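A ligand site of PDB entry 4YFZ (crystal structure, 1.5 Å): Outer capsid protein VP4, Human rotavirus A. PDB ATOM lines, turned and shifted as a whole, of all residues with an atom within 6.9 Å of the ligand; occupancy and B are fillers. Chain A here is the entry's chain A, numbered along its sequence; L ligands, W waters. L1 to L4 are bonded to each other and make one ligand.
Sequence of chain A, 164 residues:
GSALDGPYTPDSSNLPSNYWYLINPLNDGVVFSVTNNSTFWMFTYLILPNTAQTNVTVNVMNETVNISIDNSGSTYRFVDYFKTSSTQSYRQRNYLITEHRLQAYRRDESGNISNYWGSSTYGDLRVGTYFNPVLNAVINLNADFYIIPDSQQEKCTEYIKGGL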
ATOM      1  N   ARG A  77       9.949   3.011  20.851  1.00  0.00           N
ATOM      2  CA  ARG A  77      10.249   1.953  21.803  1.00  0.00           C
ATOM      3  C   ARG A  77      10.858   2.557  23.054  1.00  0.00           C
ATOM      4  O   ARG A  77      11.957   3.116  23.006  1.00  0.00           O
ATOM      5  CB  ARG A  77      11.193   0.921  21.188  1.00  0.00           C
ATOM      6  CG  ARG A  77      11.336  -0.388  21.947  1.00  0.00           C
ATOM      7  CD  ARG A  77      12.428  -1.200  21.248  1.00  0.00           C
ATOM      8  NE  ARG A  77      12.581  -2.566  21.720  1.00  0.00           N
ATOM      9  CZ  ARG A  77      12.140  -3.633  21.065  1.00  0.00           C
ATOM     10  NH1 ARG A  77      11.505  -3.488  19.908  1.00  0.00           N
ATOM     11  NH2 ARG A  77      12.342  -4.850  21.556  1.00  0.00           N
ATOM     12  N   ARG A  93      15.974  -4.461  30.235  1.00  0.00           N
ATOM     13  CA  ARG A  93      14.866  -5.230  30.780  1.00  0.00           C
ATOM     14  C   ARG A  93      13.677  -5.121  29.826  1.00  0.00           C
ATOM     15  O   ARG A  93      13.809  -5.359  28.637  1.00  0.00           O
ATOM     16  CB  ARG A  93      14.493  -4.748  32.184  1.00  0.00           C
ATOM     17  CG  ARG A  93      15.485  -5.157  33.238  1.00  0.00           C
ATOM     18  CD  ARG A  93      15.536  -6.660  33.423  1.00  0.00           C
ATOM     19  NE  ARG A  93      14.385  -7.176  34.147  1.00  0.00           N
ATOM     20  CZ  ARG A  93      14.214  -7.045  35.462  1.00  0.00           C
ATOM     21  NH1 ARG A  93      15.119  -6.404  36.186  1.00  0.00           N
ATOM     22  NH2 ARG A  93      13.132  -7.563  36.043  1.00  0.00           N
ATOM     23  N   ASN A  94      12.525  -4.713  30.349  1.00  0.00           N
ATOM     24  CA  ASN A  94      11.344  -4.668  29.502  1.00  0.00           C
ATOM     25  C   ASN A  94      11.290  -3.431  28.636  1.00  0.00           C
ATOM     26  O   ASN A  94      12.033  -2.461  28.844  1.00  0.00           O
ATOM     27  CB  ASN A  94      10.099  -4.771  30.363  1.00  0.00           C
ATOM     28  CG  ASN A  94       9.993  -6.116  31.028  1.00  0.00           C
ATOM     29  OD1 ASN A  94      10.222  -6.243  32.237  1.00  0.00           O
ATOM     30  ND2 ASN A  94       9.685  -7.133  30.241  1.00  0.00           N
ATOM     31  N   TYR A  95      10.409  -3.497  27.643  1.00  0.00           N
ATOM     32  CA  TYR A  95      10.194  -2.393  26.715  1.00  0.00           C
ATOM     33  C   TYR A  95       8.707  -2.198  26.450  1.00  0.00           C
ATOM     34  O   TYR A  95       7.891  -3.083  26.696  1.00  0.00           O
ATOM     35  CB  TYR A  95      10.926  -2.631  25.397  1.00  0.00           C
ATOM     36  CG  TYR A  95      10.601  -3.929  24.694  1.00  0.00           C
ATOM     37  CD1 TYR A  95       9.513  -4.027  23.835  1.00  0.00           C
ATOM     38  CD2 TYR A  95      11.399  -5.047  24.883  1.00  0.00           C
ATOM     39  CE1 TYR A  95       9.215  -5.218  23.196  1.00  0.00           C
ATOM     40  CE2 TYR A  95      11.103  -6.237  24.234  1.00  0.00           C
ATOM     41  CZ  TYR A  95      10.022  -6.307  23.398  1.00  0.00           C
ATOM     42  OH  TYR A  95       9.710  -7.485  22.748  1.00  0.00           O
ATOM     43  N   LEU A  96       8.394  -1.010  25.953  1.00  0.00           N
ATOM     44  CA  LEU A  96       7.060  -0.658  25.519  1.00  0.00           C
ATOM     45  C   LEU A  96       7.151  -0.211  24.073  1.00  0.00           C
ATOM     46  O   LEU A  96       7.906   0.721  23.754  1.00  0.00           O
ATOM     47  CB  LEU A  96       6.468   0.455  26.377  1.00  0.00           C
ATOM     48  CG  LEU A  96       5.171   1.082  25.881  1.00  0.00           C
ATOM     49  CD1 LEU A  96       4.031   0.094  26.017  1.00  0.00           C
ATOM     50  CD2 LEU A  96       4.851   2.362  26.645  1.00  0.00           C
ATOM     51  N   ILE A  97       6.414  -0.873  23.186  1.00  0.00           N
ATOM     52  CA  ILE A  97       6.340  -0.474  21.787  1.00  0.00           C
ATOM     53  C   ILE A  97       5.077   0.334  21.615  1.00  0.00           C
ATOM     54  O   ILE A  97       3.980  -0.139  21.944  1.00  0.00           O
ATOM     55  CB  ILE A  97       6.300  -1.694  20.863  1.00  0.00           C
ATOM     56  CG1 ILE A  97       7.601  -2.491  20.959  1.00  0.00           C
ATOM     57  CG2 ILE A  97       6.029  -1.276  19.411  1.00  0.00           C
ATOM     58  CD1 ILE A  97       7.568  -3.775  20.152  1.00  0.00           C
ATOM     59  N   TRP A 117       4.559  -2.311  29.880  1.00  0.00           N
ATOM     60  CA  TRP A 117       5.394  -3.201  29.082  1.00  0.00           C
ATOM     61  C   TRP A 117       4.590  -3.804  27.939  1.00  0.00           C
ATOM     62  O   TRP A 117       3.383  -3.975  28.040  1.00  0.00           O
ATOM     63  CB  TRP A 117       5.940  -4.374  29.923  1.00  0.00           C
ATOM     64  CG  TRP A 117       6.662  -4.035  31.184  1.00  0.00           C
ATOM     65  CD1 TRP A 117       7.109  -2.813  31.591  1.00  0.00           C
ATOM     66  CD2 TRP A 117       7.011  -4.956  32.226  1.00  0.00           C
ATOM     67  NE1 TRP A 117       7.721  -2.916  32.820  1.00  0.00           N
ATOM     68  CE2 TRP A 117       7.672  -4.220  33.232  1.00  0.00           C
ATOM     69  CE3 TRP A 117       6.840  -6.339  32.394  1.00  0.00           C
ATOM     70  CZ2 TRP A 117       8.157  -4.824  34.400  1.00  0.00           C
ATOM     71  CZ3 TRP A 117       7.318  -6.935  33.551  1.00  0.00           C
ATOM     72  CH2 TRP A 117       7.963  -6.172  34.538  1.00  0.00           C
ATOM     73  N   GLY A 118       5.270  -4.159  26.857  1.00  0.00           N
ATOM     74  CA  GLY A 118       4.590  -4.843  25.782  1.00  0.00           C
ATOM     75  C   GLY A 118       4.149  -3.915  24.669  1.00  0.00           C
ATOM     76  O   GLY A 118       4.797  -2.907  24.374  1.00  0.00           O
ATOM     77  N   SER A 119       3.023  -4.259  24.066  1.00  0.00           N
ATOM     78  CA  SER A 119       2.561  -3.578  22.868  1.00  0.00           C
ATOM     79  C   SER A 119       1.053  -3.716  22.713  1.00  0.00           C
ATOM     80  O   SER A 119       0.540  -4.836  22.650  1.00  0.00           O
ATOM     81  CB  SER A 119       3.266  -4.126  21.630  1.00  0.00           C
ATOM     82  OG  SER A 119       2.644  -3.620  20.457  1.00  0.00           O
ATOM     83  N   THR A 121      -0.646  -3.036  20.110  1.00  0.00           N
ATOM     84  CA  THR A 121      -0.969  -3.566  18.799  1.00  0.00           C
ATOM     85  C   THR A 121      -0.743  -5.085  18.760  1.00  0.00           C
ATOM     86  O   THR A 121      -1.488  -5.793  18.090  1.00  0.00           O
ATOM     87  CB  THR A 121      -0.154  -2.890  17.684  1.00  0.00           C
ATOM     88  OG1 THR A 121       1.246  -3.000  17.976  1.00  0.00           O
ATOM     89  CG2 THR A 121      -0.529  -1.410  17.580  1.00  0.00           C
ATOM     90  N   TYR A 122       0.261  -5.568  19.476  1.00  0.00           N
ATOM     91  CA  TYR A 122       0.501  -7.013  19.537  1.00  0.00           C
ATOM     92  C   TYR A 122      -0.506  -7.724  20.453  1.00  0.00           C
ATOM     93  O   TYR A 122      -0.871  -8.876  20.224  1.00  0.00           O
ATOM     94  CB  TYR A 122       1.918  -7.320  20.005  1.00  0.00           C
ATOM     95  CG  TYR A 122       2.196  -8.797  20.078  1.00  0.00           C
ATOM     96  CD1 TYR A 122       2.263  -9.562  18.925  1.00  0.00           C
ATOM     97  CD2 TYR A 122       2.384  -9.439  21.297  1.00  0.00           C
ATOM     98  CE1 TYR A 122       2.513 -10.912  18.975  1.00  0.00           C
ATOM     99  CE2 TYR A 122       2.621 -10.806  21.354  1.00  0.00           C
ATOM    100  CZ  TYR A 122       2.691 -11.535  20.195  1.00  0.00           C
ATOM    101  OH  TYR A 122       2.930 -12.885  20.224  1.00  0.00           O
ATOM    102  N   GLY A 123      -0.933  -7.038  21.514  1.00  0.00           N
ATOM    103  CA  GLY A 123      -1.968  -7.591  22.380  1.00  0.00           C
ATOM    104  C   GLY A 123      -1.507  -8.013  23.764  1.00  0.00           C
ATOM    105  O   GLY A 123      -2.239  -8.672  24.505  1.00  0.00           O
ATOM    106  N   ASP A 124      -0.284  -7.624  24.130  1.00  0.00           N
ATOM    107  CA  ASP A 124       0.213  -7.986  25.452  1.00  0.00           C
ATOM    108  C   ASP A 124       0.586  -6.764  26.305  1.00  0.00           C
ATOM    109  O   ASP A 124       1.369  -6.879  27.240  1.00  0.00           O
ATOM    110  CB  ASP A 124       1.406  -8.940  25.329  1.00  0.00           C
ATOM    111  CG  ASP A 124       2.641  -8.272  24.741  1.00  0.00           C
ATOM    112  OD1 ASP A 124       2.536  -7.145  24.202  1.00  0.00           O
ATOM    113  OD2 ASP A 124       3.738  -8.893  24.788  1.00  0.00           O
ATOM    114  N   LEU A 125      -0.001  -5.608  26.004  1.00  0.00           N
ATOM    115  CA  LEU A 125       0.216  -4.443  26.844  1.00  0.00           C
ATOM    116  C   LEU A 125      -0.191  -4.777  28.281  1.00  0.00           C
ATOM    117  O   LEU A 125      -1.254  -5.345  28.505  1.00  0.00           O
ATOM    118  CB  LEU A 125      -0.581  -3.245  26.349  1.00  0.00           C
ATOM    119  CG  LEU A 125      -0.350  -1.951  27.121  1.00  0.00           C
ATOM    120  CD1 LEU A 125       1.049  -1.422  26.893  1.00  0.00           C
ATOM    121  CD2 LEU A 125      -1.361  -0.912  26.717  1.00  0.00           C
ATOM    122  N   ARG A 126       0.675  -4.452  29.235  1.00  0.00           N
ATOM    123  CA  ARG A 126       0.416  -4.777  30.631  1.00  0.00           C
ATOM    124  C   ARG A 126       1.201  -3.836  31.529  1.00  0.00           C
ATOM    125  O   ARG A 126       2.225  -3.268  31.118  1.00  0.00           O
ATOM    126  CB  ARG A 126       0.818  -6.224  30.933  1.00  0.00           C
ATOM    127  CG  ARG A 126       2.315  -6.490  30.707  1.00  0.00           C
ATOM    128  CD  ARG A 126       2.611  -7.980  30.498  1.00  0.00           C
ATOM    129  NE  ARG A 126       4.015  -8.255  30.219  1.00  0.00           N
ATOM    130  CZ  ARG A 126       4.594  -8.158  29.024  1.00  0.00           C
ATOM    131  NH1 ARG A 126       3.913  -7.719  27.979  1.00  0.00           N
ATOM    132  NH2 ARG A 126       5.872  -8.490  28.886  1.00  0.00           N
ATOM    133  N   TYR A 130       8.742  -4.006  38.752  1.00  0.00           N
ATOM    134  CA  TYR A 130      10.100  -4.451  39.039  1.00  0.00           C
ATOM    135  C   TYR A 130      10.260  -4.581  40.554  1.00  0.00           C
ATOM    136  O   TYR A 130      10.163  -3.587  41.269  1.00  0.00           O
ATOM    137  CB  TYR A 130      11.130  -3.471  38.494  1.00  0.00           C
ATOM    138  CG  TYR A 130      11.186  -3.402  36.980  1.00  0.00           C
ATOM    139  CD1 TYR A 130      11.758  -4.435  36.248  1.00  0.00           C
ATOM    140  CD2 TYR A 130      10.693  -2.299  36.301  1.00  0.00           C
ATOM    141  CE1 TYR A 130      11.821  -4.383  34.865  1.00  0.00           C
ATOM    142  CE2 TYR A 130      10.747  -2.225  34.908  1.00  0.00           C
ATOM    143  CZ  TYR A 130      11.318  -3.274  34.196  1.00  0.00           C
ATOM    144  OH  TYR A 130      11.403  -3.241  32.824  1.00  0.00           O
HETATM  145  C1  LIG L   1       9.785 -10.720  31.518  1.00  0.00           C
HETATM  146  C2  LIG L   1       8.705 -10.639  30.474  1.00  0.00           C
HETATM  147  C3  LIG L   1       9.346 -10.900  29.112  1.00  0.00           C
HETATM  148  C4  LIG L   1      10.010 -12.286  29.169  1.00  0.00           C
HETATM  149  C5  LIG L   1      10.773 -12.629  27.886  1.00  0.00           C
HETATM  150  C6  LIG L   1      10.381 -12.101  31.486  1.00  0.00           C
HETATM  151  O1  LIG L   1      11.433 -12.209  32.444  1.00  0.00           O
HETATM  152  O2  LIG L   1       9.253 -10.438  32.804  1.00  0.00           O
HETATM  153  O3  LIG L   1       8.090  -9.332  30.506  1.00  0.00           O
HETATM  154  O4  LIG L   1       8.330 -10.913  28.107  1.00  0.00           O
HETATM  155  O5  LIG L   1      10.972 -12.305  30.225  1.00  0.00           O
HETATM  156  O6  LIG L   1      11.751 -11.617  27.590  1.00  0.00           O
HETATM  157  C1  LG2 L   2       8.604 -10.159  26.934  1.00  0.00           C
HETATM  158  C2  LG2 L   2       7.645 -10.662  25.882  1.00  0.00           C
HETATM  159  C3  LG2 L   2       7.689  -9.731  24.687  1.00  0.00           C
HETATM  160  C4  LG2 L   2       7.401  -8.280  25.147  1.00  0.00           C
HETATM  161  C5  LG2 L   2       8.454  -7.919  26.167  1.00  0.00           C
HETATM  162  C6  LG2 L   2       8.271  -6.493  26.678  1.00  0.00           C
HETATM  163  O1  LG2 L   2       8.074 -11.975  25.472  1.00  0.00           O
HETATM  164  O2  LG2 L   2       6.741 -10.196  23.731  1.00  0.00           O
HETATM  165  O3  LG2 L   2       6.088  -8.159  25.757  1.00  0.00           O
HETATM  166  O4  LG2 L   2       8.317  -8.795  27.306  1.00  0.00           O
HETATM  167  O5  LG2 L   2       9.341  -6.216  27.602  1.00  0.00           O
HETATM  168  C1  LG3 L   3       7.131 -10.077  22.363  1.00  0.00           C
HETATM  169  C2  LG3 L   3       6.432 -11.209  21.600  1.00  0.00           C
HETATM  170  C3  LG3 L   3       6.548 -11.012  20.104  1.00  0.00           C
HETATM  171  C4  LG3 L   3       6.095  -9.603  19.741  1.00  0.00           C
HETATM  172  C5  LG3 L   3       6.940  -8.624  20.529  1.00  0.00           C
HETATM  173  C6  LG3 L   3       6.648  -7.174  20.098  1.00  0.00           C
HETATM  174  C7  LG3 L   3       6.388 -13.434  22.668  1.00  0.00           C
HETATM  175  C8  LG3 L   3       7.129 -14.741  22.883  1.00  0.00           C
HETATM  176  N1  LG3 L   3       7.027 -12.517  21.938  1.00  0.00           N
HETATM  177  O1  LG3 L   3       5.663 -11.965  19.486  1.00  0.00           O
HETATM  178  O2  LG3 L   3       6.271  -9.388  18.315  1.00  0.00           O
HETATM  179  O3  LG3 L   3       6.646  -8.797  21.934  1.00  0.00           O
HETATM  180  O4  LG3 L   3       5.279  -6.859  20.294  1.00  0.00           O
HETATM  181  O5  LG3 L   3       5.260 -13.262  23.133  1.00  0.00           O
HETATM  182  C1  LG4 L   4       6.302 -12.886  18.621  1.00  0.00           C
HETATM  183  C2  LG4 L   4       5.361 -14.052  18.361  1.00  0.00           C
HETATM  184  C3  LG4 L   4       6.111 -15.074  17.521  1.00  0.00           C
HETATM  185  C4  LG4 L   4       6.572 -14.428  16.239  1.00  0.00           C
HETATM  186  C5  LG4 L   4       7.369 -13.165  16.561  1.00  0.00           C
HETATM  187  C6  LG4 L   4       7.729 -12.489  15.250  1.00  0.00           C
HETATM  188  O1  LG4 L   4       4.943 -14.611  19.615  1.00  0.00           O
HETATM  189  O2  LG4 L   4       5.249 -16.174  17.196  1.00  0.00           O
HETATM  190  O3  LG4 L   4       5.420 -14.076  15.463  1.00  0.00           O
HETATM  191  O4  LG4 L   4       6.579 -12.248  17.377  1.00  0.00           O
HETATM  192  O5  LG4 L   4       7.972 -11.102  15.455  1.00  0.00           O
HETATM  193  O   HOH W   1      13.472 -13.453  30.679  1.00  0.00           O
HETATM  194  O   HOH W   2      10.288 -14.240  34.023  1.00  0.00           O
HETATM  195  O   HOH W   3       8.938  -9.390  17.416  1.00  0.00           O
HETATM  196  O   HOH W   4       5.380 -15.102  13.060  1.00  0.00           O
HETATM  197  O   HOH W   5      12.002  -7.642  27.180  1.00  0.00           O
HETATM  198  O   HOH W   6       4.432  -7.982  16.479  1.00  0.00           O
HETATM  199  O   HOH W   7      12.885 -14.003  33.359  1.00  0.00           O
HETATM  200  O   HOH W   8       4.985  -6.767  22.886  1.00  0.00           O
HETATM  201  O   HOH W   9       2.281 -14.658  22.362  1.00  0.00           O
HETATM  202  O   HOH W  10       4.299  -4.893  18.632  1.00  0.00           O
HETATM  203  O   HOH W  11       7.116 -14.311  26.491  1.00  0.00           O
HETATM  204  O   HOH W  12      13.654 -11.469  29.251  1.00  0.00           O
HETATM  205  O   HOH W  13       4.543 -14.821  25.353  1.00  0.00           O
HETATM  206  O   HOH W  14       4.142 -11.542  25.074  1.00  0.00           O
HETATM  207  O   HOH W  15      10.821  -8.585  33.991  1.00  0.00           O
HETATM  208  O   HOH W  16      12.275  -9.694  25.703  1.00  0.00           O
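An oxygen (O3) of LG2 L2 lies within hydrogen-bond range of the side-chain carboxylate (OD2) of Asp 124 (2.6 Å). The side-chain hydroxyl of Tyr 122 is in hydrogen-bond range of an oxygen (O1) of LG4 L4 (2.7 Å). O3 of LIG L1 sits at hydrogen-bond distance from ND2 of Asn 94. O3 of LIG L1 lies within hydrogen-bond range of NH2 of Arg 126 (2.9 Å). The backbone NH of Tyr 95 lies within hydrogen-bond range of an oxygen (O5) of LG2 L2 (2.9 Å). OH of Tyr 95 sits close to O3 of LG3 L3, at 3.4 Å.
The guanidinium group (NH1) of Arg 126 is in salt-bridge range of the side-chain carboxylate (OD2) of Asp 124, 3.4 Å away. The backbone NH of Ser 119 is in hydrogen-bond range of the side-chain carboxylate of Asp 124 (2.9 Å). OG of Ser 119 sits at hydrogen-bond distance from N of Tyr 122 (3.2 Å). The backbone NH (N) of Asn 94 lies within hydrogen-bond range of the side-chain hydroxyl (OH) of Tyr 130. N of Trp 117 sits at hydrogen-bond distance from O of Arg 126, 2.8 Å away. The backbone NH of Gly 118 sits at hydrogen-bond distance from the backbone carbonyl oxygen of Tyr 95 (2.8 Å). The backbone carbonyl oxygen (O) of Gly 118 lies within hydrogen-bond range of the backbone NH (N) of Ile 97 (2.9 Å). The backbone carbonyl oxygen of Ser 119 sits at hydrogen-bond distance from the backbone NH of Leu 125 (3.5 Å).
Residues that only touch the ligand: Ile 97, Gly 118, Ser 119 and Trp 117. Hydrophobic or aromatic side chains within 4 Å of the ligand: Tyr 95, Ile 97, Trp 117 and Tyr 122. Of the 16 residues printed, 9 come within 4 Å of the ligand.
Water W8 lies within hydrogen-bond range of O4 of LG3 L3 (2.6 Å), OD1 of Asp 124 (2.8 Å) and N of Ser 119 (3.4 Å). Water W15 lies within hydrogen-bond range of an oxygen (O2) of LIG L1, the side-chain amide oxygen of Asn 94 and the guanidinium group of Arg 93. Water W10 bridges an oxygen (O4) of LG3 L3 and the side-chain hydroxyl (OG) of Ser 119. Water W14 lies within hydrogen-bond range of the side-chain carboxylate of Asp 124 and an oxygen (O5) of LG3 L3. Water W5 lies within hydrogen-bond range of O5 of LG2 L2 (3.0 Å) and O of Arg 93 (3.3 Å). Water W9 lies within hydrogen-bond range of OH of Tyr 122 (2.9 Å) and O5 of LG3 L3 (3.4 Å).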
